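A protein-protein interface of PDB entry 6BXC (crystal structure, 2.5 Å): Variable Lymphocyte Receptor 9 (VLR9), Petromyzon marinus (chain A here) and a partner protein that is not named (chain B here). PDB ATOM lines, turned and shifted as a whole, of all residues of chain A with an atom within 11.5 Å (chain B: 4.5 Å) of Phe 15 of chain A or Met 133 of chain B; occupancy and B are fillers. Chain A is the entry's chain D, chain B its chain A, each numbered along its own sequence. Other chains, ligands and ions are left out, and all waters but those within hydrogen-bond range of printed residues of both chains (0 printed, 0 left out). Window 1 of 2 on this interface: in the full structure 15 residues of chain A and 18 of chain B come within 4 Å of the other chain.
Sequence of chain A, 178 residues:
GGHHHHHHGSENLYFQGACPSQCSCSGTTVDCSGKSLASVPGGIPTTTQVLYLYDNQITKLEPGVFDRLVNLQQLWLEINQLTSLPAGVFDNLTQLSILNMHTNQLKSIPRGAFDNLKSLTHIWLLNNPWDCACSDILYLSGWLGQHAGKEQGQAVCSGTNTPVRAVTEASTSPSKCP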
ATOM      1  N   LEU A  13     -15.954 -16.409  -2.250  1.00  0.00           N
ATOM      2  CA  LEU A  13     -15.946 -15.510  -1.094  1.00  0.00           C
ATOM      3  C   LEU A  13     -15.722 -16.264   0.214  1.00  0.00           C
ATOM      4  O   LEU A  13     -14.853 -15.908   1.010  1.00  0.00           O
ATOM      5  CB  LEU A  13     -17.252 -14.717  -1.000  1.00  0.00           C
ATOM      6  CG  LEU A  13     -17.246 -13.710   0.160  1.00  0.00           C
ATOM      7  CD1 LEU A  13     -16.387 -12.489  -0.166  1.00  0.00           C
ATOM      8  CD2 LEU A  13     -18.655 -13.288   0.560  1.00  0.00           C
ATOM      9  N   TYR A  14     -16.526 -17.293   0.459  1.00  0.00           N
ATOM     10  CA  TYR A  14     -16.239 -18.205   1.554  1.00  0.00           C
ATOM     11  C   TYR A  14     -15.711 -19.551   1.096  1.00  0.00           C
ATOM     12  O   TYR A  14     -14.935 -20.171   1.823  1.00  0.00           O
ATOM     13  CB  TYR A  14     -17.483 -18.415   2.427  1.00  0.00           C
ATOM     14  CG  TYR A  14     -17.694 -17.263   3.377  1.00  0.00           C
ATOM     15  CD1 TYR A  14     -16.733 -16.950   4.337  1.00  0.00           C
ATOM     16  CD2 TYR A  14     -18.833 -16.476   3.304  1.00  0.00           C
ATOM     17  CE1 TYR A  14     -16.905 -15.887   5.198  1.00  0.00           C
ATOM     18  CE2 TYR A  14     -19.016 -15.411   4.164  1.00  0.00           C
ATOM     19  CZ  TYR A  14     -18.056 -15.121   5.109  1.00  0.00           C
ATOM     20  OH  TYR A  14     -18.245 -14.061   5.967  1.00  0.00           O
ATOM     21  N   PHE A  15     -16.096 -20.005  -0.095  1.00  0.00           N
ATOM     22  CA  PHE A  15     -15.679 -21.306  -0.589  1.00  0.00           C
ATOM     23  C   PHE A  15     -15.322 -21.191  -2.061  1.00  0.00           C
ATOM     24  O   PHE A  15     -16.043 -20.550  -2.833  1.00  0.00           O
ATOM     25  CB  PHE A  15     -16.776 -22.352  -0.370  1.00  0.00           C
ATOM     26  CG  PHE A  15     -17.031 -22.660   1.080  1.00  0.00           C
ATOM     27  CD1 PHE A  15     -17.883 -21.871   1.832  1.00  0.00           C
ATOM     28  CD2 PHE A  15     -16.404 -23.731   1.694  1.00  0.00           C
ATOM     29  CE1 PHE A  15     -18.105 -22.142   3.166  1.00  0.00           C
ATOM     30  CE2 PHE A  15     -16.631 -24.014   3.031  1.00  0.00           C
ATOM     31  CZ  PHE A  15     -17.484 -23.211   3.765  1.00  0.00           C
ATOM     32  N   GLN A  16     -14.184 -21.778  -2.426  1.00  0.00           N
ATOM     33  CA  GLN A  16     -13.767 -21.962  -3.813  1.00  0.00           C
ATOM     34  C   GLN A  16     -13.884 -23.458  -4.075  1.00  0.00           C
ATOM     35  O   GLN A  16     -12.946 -24.220  -3.833  1.00  0.00           O
ATOM     36  CB  GLN A  16     -12.340 -21.451  -4.058  1.00  0.00           C
ATOM     37  CG  GLN A  16     -12.133 -19.957  -3.794  1.00  0.00           C
ATOM     38  CD  GLN A  16     -10.671 -19.535  -3.935  1.00  0.00           C
ATOM     39  N   GLY A  17     -15.046 -23.881  -4.557  1.00  0.00           N
ATOM     40  CA  GLY A  17     -15.364 -25.301  -4.529  1.00  0.00           C
ATOM     41  C   GLY A  17     -15.751 -25.702  -3.121  1.00  0.00           C
ATOM     42  O   GLY A  17     -16.640 -25.095  -2.525  1.00  0.00           O
ATOM     43  N   ALA A  18     -15.079 -26.712  -2.569  1.00  0.00           N
ATOM     44  CA  ALA A  18     -15.258 -27.105  -1.175  1.00  0.00           C
ATOM     45  C   ALA A  18     -14.137 -26.600  -0.281  1.00  0.00           C
ATOM     46  O   ALA A  18     -14.176 -26.817   0.936  1.00  0.00           O
ATOM     47  CB  ALA A  18     -15.357 -28.628  -1.055  1.00  0.00           C
ATOM     48  N   CYS A  19     -13.152 -25.944  -0.857  1.00  0.00           N
ATOM     49  CA  CYS A  19     -12.049 -25.392  -0.096  1.00  0.00           C
ATOM     50  C   CYS A  19     -12.422 -24.052   0.516  1.00  0.00           C
ATOM     51  O   CYS A  19     -13.007 -23.208  -0.171  1.00  0.00           O
ATOM     52  CB  CYS A  19     -10.845 -25.205  -1.009  1.00  0.00           C
ATOM     53  SG  CYS A  19      -9.317 -24.822  -0.180  1.00  0.00           S
ATOM     54  N   PRO A  20     -12.131 -23.829   1.795  1.00  0.00           N
ATOM     55  CA  PRO A  20     -12.363 -22.501   2.369  1.00  0.00           C
ATOM     56  C   PRO A  20     -11.608 -21.450   1.567  1.00  0.00           C
ATOM     57  O   PRO A  20     -10.476 -21.666   1.140  1.00  0.00           O
ATOM     58  CB  PRO A  20     -11.822 -22.631   3.795  1.00  0.00           C
ATOM     59  CG  PRO A  20     -11.938 -24.083   4.096  1.00  0.00           C
ATOM     60  CD  PRO A  20     -11.642 -24.785   2.800  1.00  0.00           C
ATOM     61  N   SER A  21     -12.261 -20.318   1.333  1.00  0.00           N
ATOM     62  CA  SER A  21     -11.714 -19.319   0.419  1.00  0.00           C
ATOM     63  C   SER A  21     -10.372 -18.784   0.901  1.00  0.00           C
ATOM     64  O   SER A  21      -9.526 -18.408   0.081  1.00  0.00           O
ATOM     65  CB  SER A  21     -12.714 -18.183   0.202  1.00  0.00           C
ATOM     66  OG  SER A  21     -13.001 -17.511   1.409  1.00  0.00           O
ATOM     67  N   GLN A  22     -10.142 -18.767   2.218  1.00  0.00           N
ATOM     68  CA  GLN A  22      -8.877 -18.275   2.749  1.00  0.00           C
ATOM     69  C   GLN A  22      -7.754 -19.294   2.631  1.00  0.00           C
ATOM     70  O   GLN A  22      -6.590 -18.948   2.872  1.00  0.00           O
ATOM     71  CB  GLN A  22      -9.072 -17.905   4.220  1.00  0.00           C
ATOM     72  CG  GLN A  22      -9.904 -16.654   4.438  1.00  0.00           C
ATOM     73  CD  GLN A  22     -10.573 -16.636   5.801  1.00  0.00           C
ATOM     74  OE1 GLN A  22     -11.037 -17.671   6.285  1.00  0.00           O
ATOM     75  NE2 GLN A  22     -10.640 -15.461   6.420  1.00  0.00           N
ATOM     76  N   CYS A  23      -8.066 -20.540   2.304  1.00  0.00           N
ATOM     77  CA  CYS A  23      -7.063 -21.587   2.269  1.00  0.00           C
ATOM     78  C   CYS A  23      -6.870 -22.082   0.843  1.00  0.00           C
ATOM     79  O   CYS A  23      -7.615 -21.732  -0.078  1.00  0.00           O
ATOM     80  CB  CYS A  23      -7.415 -22.736   3.216  1.00  0.00           C
ATOM     81  SG  CYS A  23      -7.907 -22.167   4.820  1.00  0.00           S
ATOM     82  N   SER A  24      -5.856 -22.927   0.679  1.00  0.00           N
ATOM     83  CA  SER A  24      -5.556 -23.586  -0.583  1.00  0.00           C
ATOM     84  C   SER A  24      -5.644 -25.086  -0.341  1.00  0.00           C
ATOM     85  O   SER A  24      -5.097 -25.586   0.648  1.00  0.00           O
ATOM     86  CB  SER A  24      -4.173 -23.185  -1.095  1.00  0.00           C
ATOM     87  OG  SER A  24      -3.869 -23.841  -2.309  1.00  0.00           O
ATOM     88  N   CYS A  25      -6.353 -25.795  -1.215  1.00  0.00           N
ATOM     89  CA  CYS A  25      -6.611 -27.212  -1.013  1.00  0.00           C
ATOM     90  C   CYS A  25      -6.121 -28.031  -2.195  1.00  0.00           C
ATOM     91  O   CYS A  25      -6.279 -27.631  -3.353  1.00  0.00           O
ATOM     92  CB  CYS A  25      -8.100 -27.469  -0.816  1.00  0.00           C
ATOM     93  SG  CYS A  25      -8.846 -26.638   0.596  1.00  0.00           S
ATOM     94  N   VAL A  30      -5.231 -29.393   3.248  1.00  0.00           N
ATOM     95  CA  VAL A  30      -5.830 -28.066   3.349  1.00  0.00           C
ATOM     96  C   VAL A  30      -4.759 -27.162   3.938  1.00  0.00           C
ATOM     97  O   VAL A  30      -4.284 -27.402   5.057  1.00  0.00           O
ATOM     98  CB  VAL A  30      -7.107 -28.069   4.212  1.00  0.00           C
ATOM     99  CG1 VAL A  30      -7.618 -26.652   4.423  1.00  0.00           C
ATOM    100  CG2 VAL A  30      -8.186 -28.900   3.543  1.00  0.00           C
ATOM    101  N   CYS A  32      -3.940 -23.592   5.164  1.00  0.00           N
ATOM    102  CA  CYS A  32      -4.381 -22.287   5.640  1.00  0.00           C
ATOM    103  C   CYS A  32      -3.244 -21.471   6.248  1.00  0.00           C
ATOM    104  O   CYS A  32      -3.493 -20.536   7.015  1.00  0.00           O
ATOM    105  CB  CYS A  32      -5.517 -22.456   6.657  1.00  0.00           C
ATOM    106  SG  CYS A  32      -6.941 -23.435   6.075  1.00  0.00           S
ATOM    107  N   SER A  39      -8.566 -17.067  13.355  1.00  0.00           N
ATOM    108  CA  SER A  39      -9.289 -18.228  13.855  1.00  0.00           C
ATOM    109  C   SER A  39      -9.211 -19.331  12.808  1.00  0.00           C
ATOM    110  O   SER A  39      -8.869 -19.096  11.647  1.00  0.00           O
ATOM    111  CB  SER A  39     -10.748 -17.896  14.213  1.00  0.00           C
ATOM    112  OG  SER A  39     -11.470 -17.383  13.108  1.00  0.00           O
ATOM    113  N   VAL A  40      -9.569 -20.535  13.224  1.00  0.00           N
ATOM    114  CA  VAL A  40      -9.578 -21.683  12.310  1.00  0.00           C
ATOM    115  C   VAL A  40     -10.719 -21.531  11.311  1.00  0.00           C
ATOM    116  O   VAL A  40     -11.856 -21.243  11.712  1.00  0.00           O
ATOM    117  CB  VAL A  40      -9.693 -22.980  13.100  1.00  0.00           C
ATOM    118  CG1 VAL A  40      -9.762 -24.162  12.158  1.00  0.00           C
ATOM    119  CG2 VAL A  40      -8.505 -23.106  14.023  1.00  0.00           C
ATOM    120  N   PRO A  41     -10.472 -21.692  10.016  1.00  0.00           N
ATOM    121  CA  PRO A  41     -11.566 -21.584   9.044  1.00  0.00           C
ATOM    122  C   PRO A  41     -12.612 -22.672   9.236  1.00  0.00           C
ATOM    123  O   PRO A  41     -12.309 -23.802   9.625  1.00  0.00           O
ATOM    124  CB  PRO A  41     -10.853 -21.737   7.694  1.00  0.00           C
ATOM    125  CG  PRO A  41      -9.446 -21.301   7.963  1.00  0.00           C
ATOM    126  CD  PRO A  41      -9.155 -21.785   9.358  1.00  0.00           C
ATOM    127  N   GLY A  42     -13.867 -22.308   8.961  1.00  0.00           N
ATOM    128  CA  GLY A  42     -14.931 -23.286   8.924  1.00  0.00           C
ATOM    129  C   GLY A  42     -14.990 -24.022   7.601  1.00  0.00           C
ATOM    130  O   GLY A  42     -14.416 -23.602   6.600  1.00  0.00           O
ATOM    131  N   GLY A  43     -15.705 -25.142   7.598  1.00  0.00           N
ATOM    132  CA  GLY A  43     -15.939 -25.855   6.359  1.00  0.00           C
ATOM    133  C   GLY A  43     -14.747 -26.626   5.845  1.00  0.00           C
ATOM    134  O   GLY A  43     -14.688 -26.933   4.649  1.00  0.00           O
ATOM    135  N   ILE A  44     -13.810 -26.979   6.711  1.00  0.00           N
ATOM    136  CA  ILE A  44     -12.700 -27.851   6.309  1.00  0.00           C
ATOM    137  C   ILE A  44     -13.256 -29.237   6.013  1.00  0.00           C
ATOM    138  O   ILE A  44     -13.966 -29.806   6.860  1.00  0.00           O
ATOM    139  CB  ILE A  44     -11.641 -27.904   7.408  1.00  0.00           C
ATOM    140  CG1 ILE A  44     -11.007 -26.528   7.597  1.00  0.00           C
ATOM    141  CG2 ILE A  44     -10.566 -28.917   7.058  1.00  0.00           C
ATOM    142  CD1 ILE A  44     -10.206 -26.396   8.860  1.00  0.00           C
ATOM    143  N   PRO A  45     -12.986 -29.811   4.845  1.00  0.00           N
ATOM    144  CA  PRO A  45     -13.643 -31.070   4.481  1.00  0.00           C
ATOM    145  C   PRO A  45     -13.252 -32.180   5.445  1.00  0.00           C
ATOM    146  O   PRO A  45     -12.132 -32.234   5.955  1.00  0.00           O
ATOM    147  CB  PRO A  45     -13.119 -31.348   3.067  1.00  0.00           C
ATOM    148  CG  PRO A  45     -12.719 -30.005   2.543  1.00  0.00           C
ATOM    149  CD  PRO A  45     -12.191 -29.259   3.735  1.00  0.00           C
ATOM    150  N   THR A  46     -14.206 -33.071   5.696  1.00  0.00           N
ATOM    151  CA  THR A  46     -13.977 -34.175   6.619  1.00  0.00           C
ATOM    152  C   THR A  46     -12.955 -35.177   6.104  1.00  0.00           C
ATOM    153  O   THR A  46     -12.417 -35.951   6.901  1.00  0.00           O
ATOM    154  CB  THR A  46     -15.293 -34.888   6.903  1.00  0.00           C
ATOM    155  OG1 THR A  46     -15.819 -35.408   5.678  1.00  0.00           O
ATOM    156  CG2 THR A  46     -16.295 -33.900   7.476  1.00  0.00           C
ATOM    157  N   THR A  48     -10.049 -34.372   5.158  1.00  0.00           N
ATOM    158  CA  THR A  48      -8.726 -33.782   5.281  1.00  0.00           C
ATOM    159  C   THR A  48      -7.823 -34.681   6.113  1.00  0.00           C
ATOM    160  O   THR A  48      -8.179 -35.104   7.219  1.00  0.00           O
ATOM    161  CB  THR A  48      -8.828 -32.388   5.901  1.00  0.00           C
ATOM    162  OG1 THR A  48      -9.632 -31.556   5.058  1.00  0.00           O
ATOM    163  CG2 THR A  48      -7.454 -31.755   6.050  1.00  0.00           C
ATOM    164  N   LEU A  69     -12.684 -33.842  12.349  1.00  0.00           N
ATOM    165  CA  LEU A  69     -11.550 -34.149  11.486  1.00  0.00           C
ATOM    166  C   LEU A  69     -10.877 -35.469  11.884  1.00  0.00           C
ATOM    167  O   LEU A  69      -9.693 -35.532  12.207  1.00  0.00           O
ATOM    168  CB  LEU A  69     -10.586 -32.972  11.530  1.00  0.00           C
ATOM    169  CG  LEU A  69     -11.338 -31.676  11.169  1.00  0.00           C
ATOM    170  CD1 LEU A  69     -10.431 -30.469  11.173  1.00  0.00           C
ATOM    171  CD2 LEU A  69     -12.047 -31.807   9.821  1.00  0.00           C
ATOM    172  N   PHE B  58     -20.969 -31.954  -0.271  1.00  0.00           N
ATOM    173  CA  PHE B  58     -21.034 -30.569  -0.734  1.00  0.00           C
ATOM    174  C   PHE B  58     -22.060 -30.434  -1.851  1.00  0.00           C
ATOM    175  O   PHE B  58     -21.905 -31.051  -2.911  1.00  0.00           O
ATOM    176  CB  PHE B  58     -19.653 -30.076  -1.200  1.00  0.00           C
ATOM    177  CG  PHE B  58     -19.584 -28.586  -1.449  1.00  0.00           C
ATOM    178  CD1 PHE B  58     -20.054 -28.038  -2.632  1.00  0.00           C
ATOM    179  CD2 PHE B  58     -19.041 -27.735  -0.496  1.00  0.00           C
ATOM    180  CE1 PHE B  58     -19.996 -26.683  -2.851  1.00  0.00           C
ATOM    181  CE2 PHE B  58     -18.982 -26.376  -0.718  1.00  0.00           C
ATOM    182  CZ  PHE B  58     -19.465 -25.852  -1.893  1.00  0.00           C
ATOM    183  N   ILE B  83     -21.721 -28.849   3.785  1.00  0.00           N
ATOM    184  CA  ILE B  83     -21.940 -27.528   3.207  1.00  0.00           C
ATOM    185  C   ILE B  83     -23.097 -27.590   2.221  1.00  0.00           C
ATOM    186  O   ILE B  83     -23.116 -28.441   1.325  1.00  0.00           O
ATOM    187  CB  ILE B  83     -20.677 -26.977   2.508  1.00  0.00           C
ATOM    188  CG1 ILE B  83     -19.470 -26.981   3.445  1.00  0.00           C
ATOM    189  CG2 ILE B  83     -20.935 -25.582   1.969  1.00  0.00           C
ATOM    190  CD1 ILE B  83     -18.545 -28.163   3.277  1.00  0.00           C
ATOM    191  N   GLU B 106     -22.775 -28.078   8.765  1.00  0.00           N
ATOM    192  CA  GLU B 106     -21.956 -27.050   9.396  1.00  0.00           C
ATOM    193  C   GLU B 106     -22.036 -25.707   8.686  1.00  0.00           C
ATOM    194  O   GLU B 106     -21.857 -24.676   9.339  1.00  0.00           O
ATOM    195  CB  GLU B 106     -20.485 -27.460   9.551  1.00  0.00           C
ATOM    196  CG  GLU B 106     -20.257 -28.771  10.264  1.00  0.00           C
ATOM    197  CD  GLU B 106     -18.801 -29.182  10.223  1.00  0.00           C
ATOM    198  OE1 GLU B 106     -17.984 -28.356   9.755  1.00  0.00           O
ATOM    199  OE2 GLU B 106     -18.470 -30.296  10.697  1.00  0.00           O
ATOM    200  N   VAL B 107     -22.268 -25.682   7.372  1.00  0.00           N
ATOM    201  CA  VAL B 107     -22.281 -24.437   6.608  1.00  0.00           C
ATOM    202  C   VAL B 107     -23.560 -24.381   5.781  1.00  0.00           C
ATOM    203  O   VAL B 107     -23.854 -25.300   5.009  1.00  0.00           O
ATOM    204  CB  VAL B 107     -21.046 -24.318   5.695  1.00  0.00           C
ATOM    205  CG1 VAL B 107     -21.065 -23.002   4.927  1.00  0.00           C
ATOM    206  CG2 VAL B 107     -19.761 -24.473   6.513  1.00  0.00           C
ATOM    207  N   LEU B 108     -24.305 -23.292   5.930  1.00  0.00           N
ATOM    208  CA  LEU B 108     -25.507 -23.006   5.157  1.00  0.00           C
ATOM    209  C   LEU B 108     -25.443 -21.594   4.611  1.00  0.00           C
ATOM    210  O   LEU B 108     -25.244 -20.643   5.374  1.00  0.00           O
ATOM    211  CB  LEU B 108     -26.777 -23.169   5.988  1.00  0.00           C
ATOM    212  CG  LEU B 108     -28.069 -22.827   5.243  1.00  0.00           C
ATOM    213  CD1 LEU B 108     -28.277 -23.659   3.990  1.00  0.00           C
ATOM    214  CD2 LEU B 108     -29.222 -23.046   6.204  1.00  0.00           C
ATOM    215  N   LEU B 131     -24.762 -26.809  13.164  1.00  0.00           N
ATOM    216  CA  LEU B 131     -24.453 -25.676  12.306  1.00  0.00           C
ATOM    217  C   LEU B 131     -23.409 -24.768  12.944  1.00  0.00           C
ATOM    218  O   LEU B 131     -23.511 -24.408  14.120  1.00  0.00           O
ATOM    219  CB  LEU B 131     -25.730 -24.903  11.992  1.00  0.00           C
ATOM    220  CG  LEU B 131     -25.660 -23.909  10.843  1.00  0.00           C
ATOM    221  CD1 LEU B 131     -25.395 -24.672   9.552  1.00  0.00           C
ATOM    222  CD2 LEU B 131     -26.956 -23.137  10.741  1.00  0.00           C
ATOM    223  N   GLU B 132     -22.431 -24.363  12.142  1.00  0.00           N
ATOM    224  CA  GLU B 132     -21.318 -23.522  12.555  1.00  0.00           C
ATOM    225  C   GLU B 132     -21.289 -22.186  11.839  1.00  0.00           C
ATOM    226  O   GLU B 132     -20.891 -21.181  12.441  1.00  0.00           O
ATOM    227  CB  GLU B 132     -19.967 -24.226  12.320  1.00  0.00           C
ATOM    228  CG  GLU B 132     -19.714 -25.489  13.123  1.00  0.00           C
ATOM    229  CD  GLU B 132     -18.326 -26.054  12.869  1.00  0.00           C
ATOM    230  OE1 GLU B 132     -17.608 -25.495  12.014  1.00  0.00           O
ATOM    231  OE2 GLU B 132     -17.942 -27.031  13.543  1.00  0.00           O
ATOM    232  N   MET B 133     -21.662 -22.150  10.559  1.00  0.00           N
ATOM    233  CA  MET B 133     -21.535 -20.954   9.734  1.00  0.00           C
ATOM    234  C   MET B 133     -22.816 -20.740   8.947  1.00  0.00           C
ATOM    235  O   MET B 133     -23.231 -21.616   8.183  1.00  0.00           O
ATOM    236  CB  MET B 133     -20.348 -21.109   8.784  1.00  0.00           C
ATOM    237  CG  MET B 133     -20.034 -19.909   7.946  1.00  0.00           C
ATOM    238  SD  MET B 133     -18.491 -20.151   7.065  1.00  0.00           S
ATOM    239  CE  MET B 133     -19.012 -19.574   5.459  1.00  0.00           C
ATOM    240  N   LEU B 134     -23.414 -19.559   9.086  1.00  0.00           N
ATOM    241  CA  LEU B 134     -24.672 -19.245   8.411  1.00  0.00           C
ATOM    242  C   LEU B 134     -24.487 -17.930   7.671  1.00  0.00           C
ATOM    243  O   LEU B 134     -24.196 -16.903   8.290  1.00  0.00           O
ATOM    244  CB  LEU B 134     -25.832 -19.177   9.408  1.00  0.00           C
ATOM    245  CG  LEU B 134     -27.236 -18.826   8.910  1.00  0.00           C
ATOM    246  CD1 LEU B 134     -27.730 -19.799   7.835  1.00  0.00           C
ATOM    247  CD2 LEU B 134     -28.204 -18.770  10.078  1.00  0.00           C
ATOM    248  N   VAL B 135     -24.647 -17.966   6.352  1.00  0.00           N
ATOM    249  CA  VAL B 135     -24.463 -16.799   5.490  1.00  0.00           C
ATOM    250  C   VAL B 135     -25.824 -16.404   4.951  1.00  0.00           C
ATOM    251  O   VAL B 135     -26.475 -17.194   4.252  1.00  0.00           O
ATOM    252  CB  VAL B 135     -23.478 -17.093   4.341  1.00  0.00           C
ATOM    253  CG1 VAL B 135     -23.280 -15.876   3.459  1.00  0.00           C
ATOM    254  CG2 VAL B 135     -22.146 -17.585   4.889  1.00  0.00           C
ATOM    255  N   VAL B 158     -20.208 -18.431  13.144  1.00  0.00           N
ATOM    256  CA  VAL B 158     -20.060 -17.496  12.028  1.00  0.00           C
ATOM    257  C   VAL B 158     -21.429 -17.112  11.493  1.00  0.00           C
ATOM    258  O   VAL B 158     -22.188 -17.980  11.047  1.00  0.00           O
ATOM    259  CB  VAL B 158     -19.184 -18.053  10.886  1.00  0.00           C
ATOM    260  CG1 VAL B 158     -19.161 -17.077   9.732  1.00  0.00           C
ATOM    261  CG2 VAL B 158     -17.755 -18.294  11.361  1.00  0.00           C
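O of Glu 106 of chain B sits at hydrogen-bond distance from N of Met 133 of chain B (2.8 Å). The backbone NH of Leu 108 of chain B is in hydrogen-bond range of the backbone carbonyl oxygen of Met 133 of chain B (3.0 Å). The backbone carbonyl oxygen of Leu 108 of chain B lies within hydrogen-bond range of the backbone NH of Val 135 of chain B, 2.9 Å away. The backbone carbonyl oxygen (O) of Tyr 14 of chain A sits at hydrogen-bond distance from the backbone NH (N) of Ser 21 of chain A (2.7 Å). SG of Cys 19 of chain A forms a disulfide with SG of Cys 25 of chain A. The side-chain sulfur of Cys 23 of chain A forms a disulfide with the side-chain sulfur of Cys 32 of chain A (2.0 Å).
Hydrophobic or aromatic side chains of chain B that line the printed part of chain A: Phe 58, Val 107, Met 133 and Val 135. Of the 25 printed residues of chain A, 4 touch a printed residue of chain B. Printed residues of chain A that touch a printed residue of chain B: Tyr 14, Phe 15, Gly 17 and Ala 18. Among the printed residues, no Asp or Glu carboxylate lies within 4 Å of a Lys or Arg side-chain nitrogen of the other chain.
Printed residues of chain B within 4 Å of Tyr 14 of chain A: Met 133 (3.4 Å) and Val 135 (3.8 Å). Of the printed residues of chain B, Phe 15 of chain A touches Val 107 (3.5 Å) and Met 133 (3.6 Å). Of the printed residues of chain B, Gly 17 of chain A touches Phe 58. Printed residues of chain B within 4 Å of Ala 18 of chain A: Phe 58 (3.8 Å). Pro 20 of chain A touches none of the printed residues of chain B. Cys 32 of chain A touches none of the printed residues of chain B. Of the printed residues of chain A, Phe 58 of chain B touches Gly 17 (3.0 Å) and Ala 18 (3.8 Å). No residue of chain A comes within 4 Å of Leu 108 of chain B. No residue of chain A comes within 4 Å of Leu 131 of chain B. Glu 132 of chain B touches none of the printed residues of chain A. Of chain A, only Tyr 14 and Phe 15 come within 4 Å of Met 133 of chain B. No residue of chain A comes within 4 Å of Val 158 of chain B. The nearest residue of chain B that does not touch Phe 15 of chain A is Ile 83 of chain B (4.1 Å). The nearest residue of chain A that does not touch Met 133 of chain B is Gly 42 of chain A (5.1 Å). The nearest printed residue of chain B that does not touch Tyr 14 of chain A is Val 158 of chain B (4.9 Å).
Among the printed residues, pairs that only touch across the chains: Tyr 14 of chain A with Met 133 of chain B, Tyr 14 of chain A with Val 135 of chain B, Phe 15 of chain A with Val 107 of chain B, Phe 15 of chain A with Met 133 of chain B, Gly 17 of chain A with Phe 58 of chain B and Ala 18 of chain A with Phe 58 of chain B.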
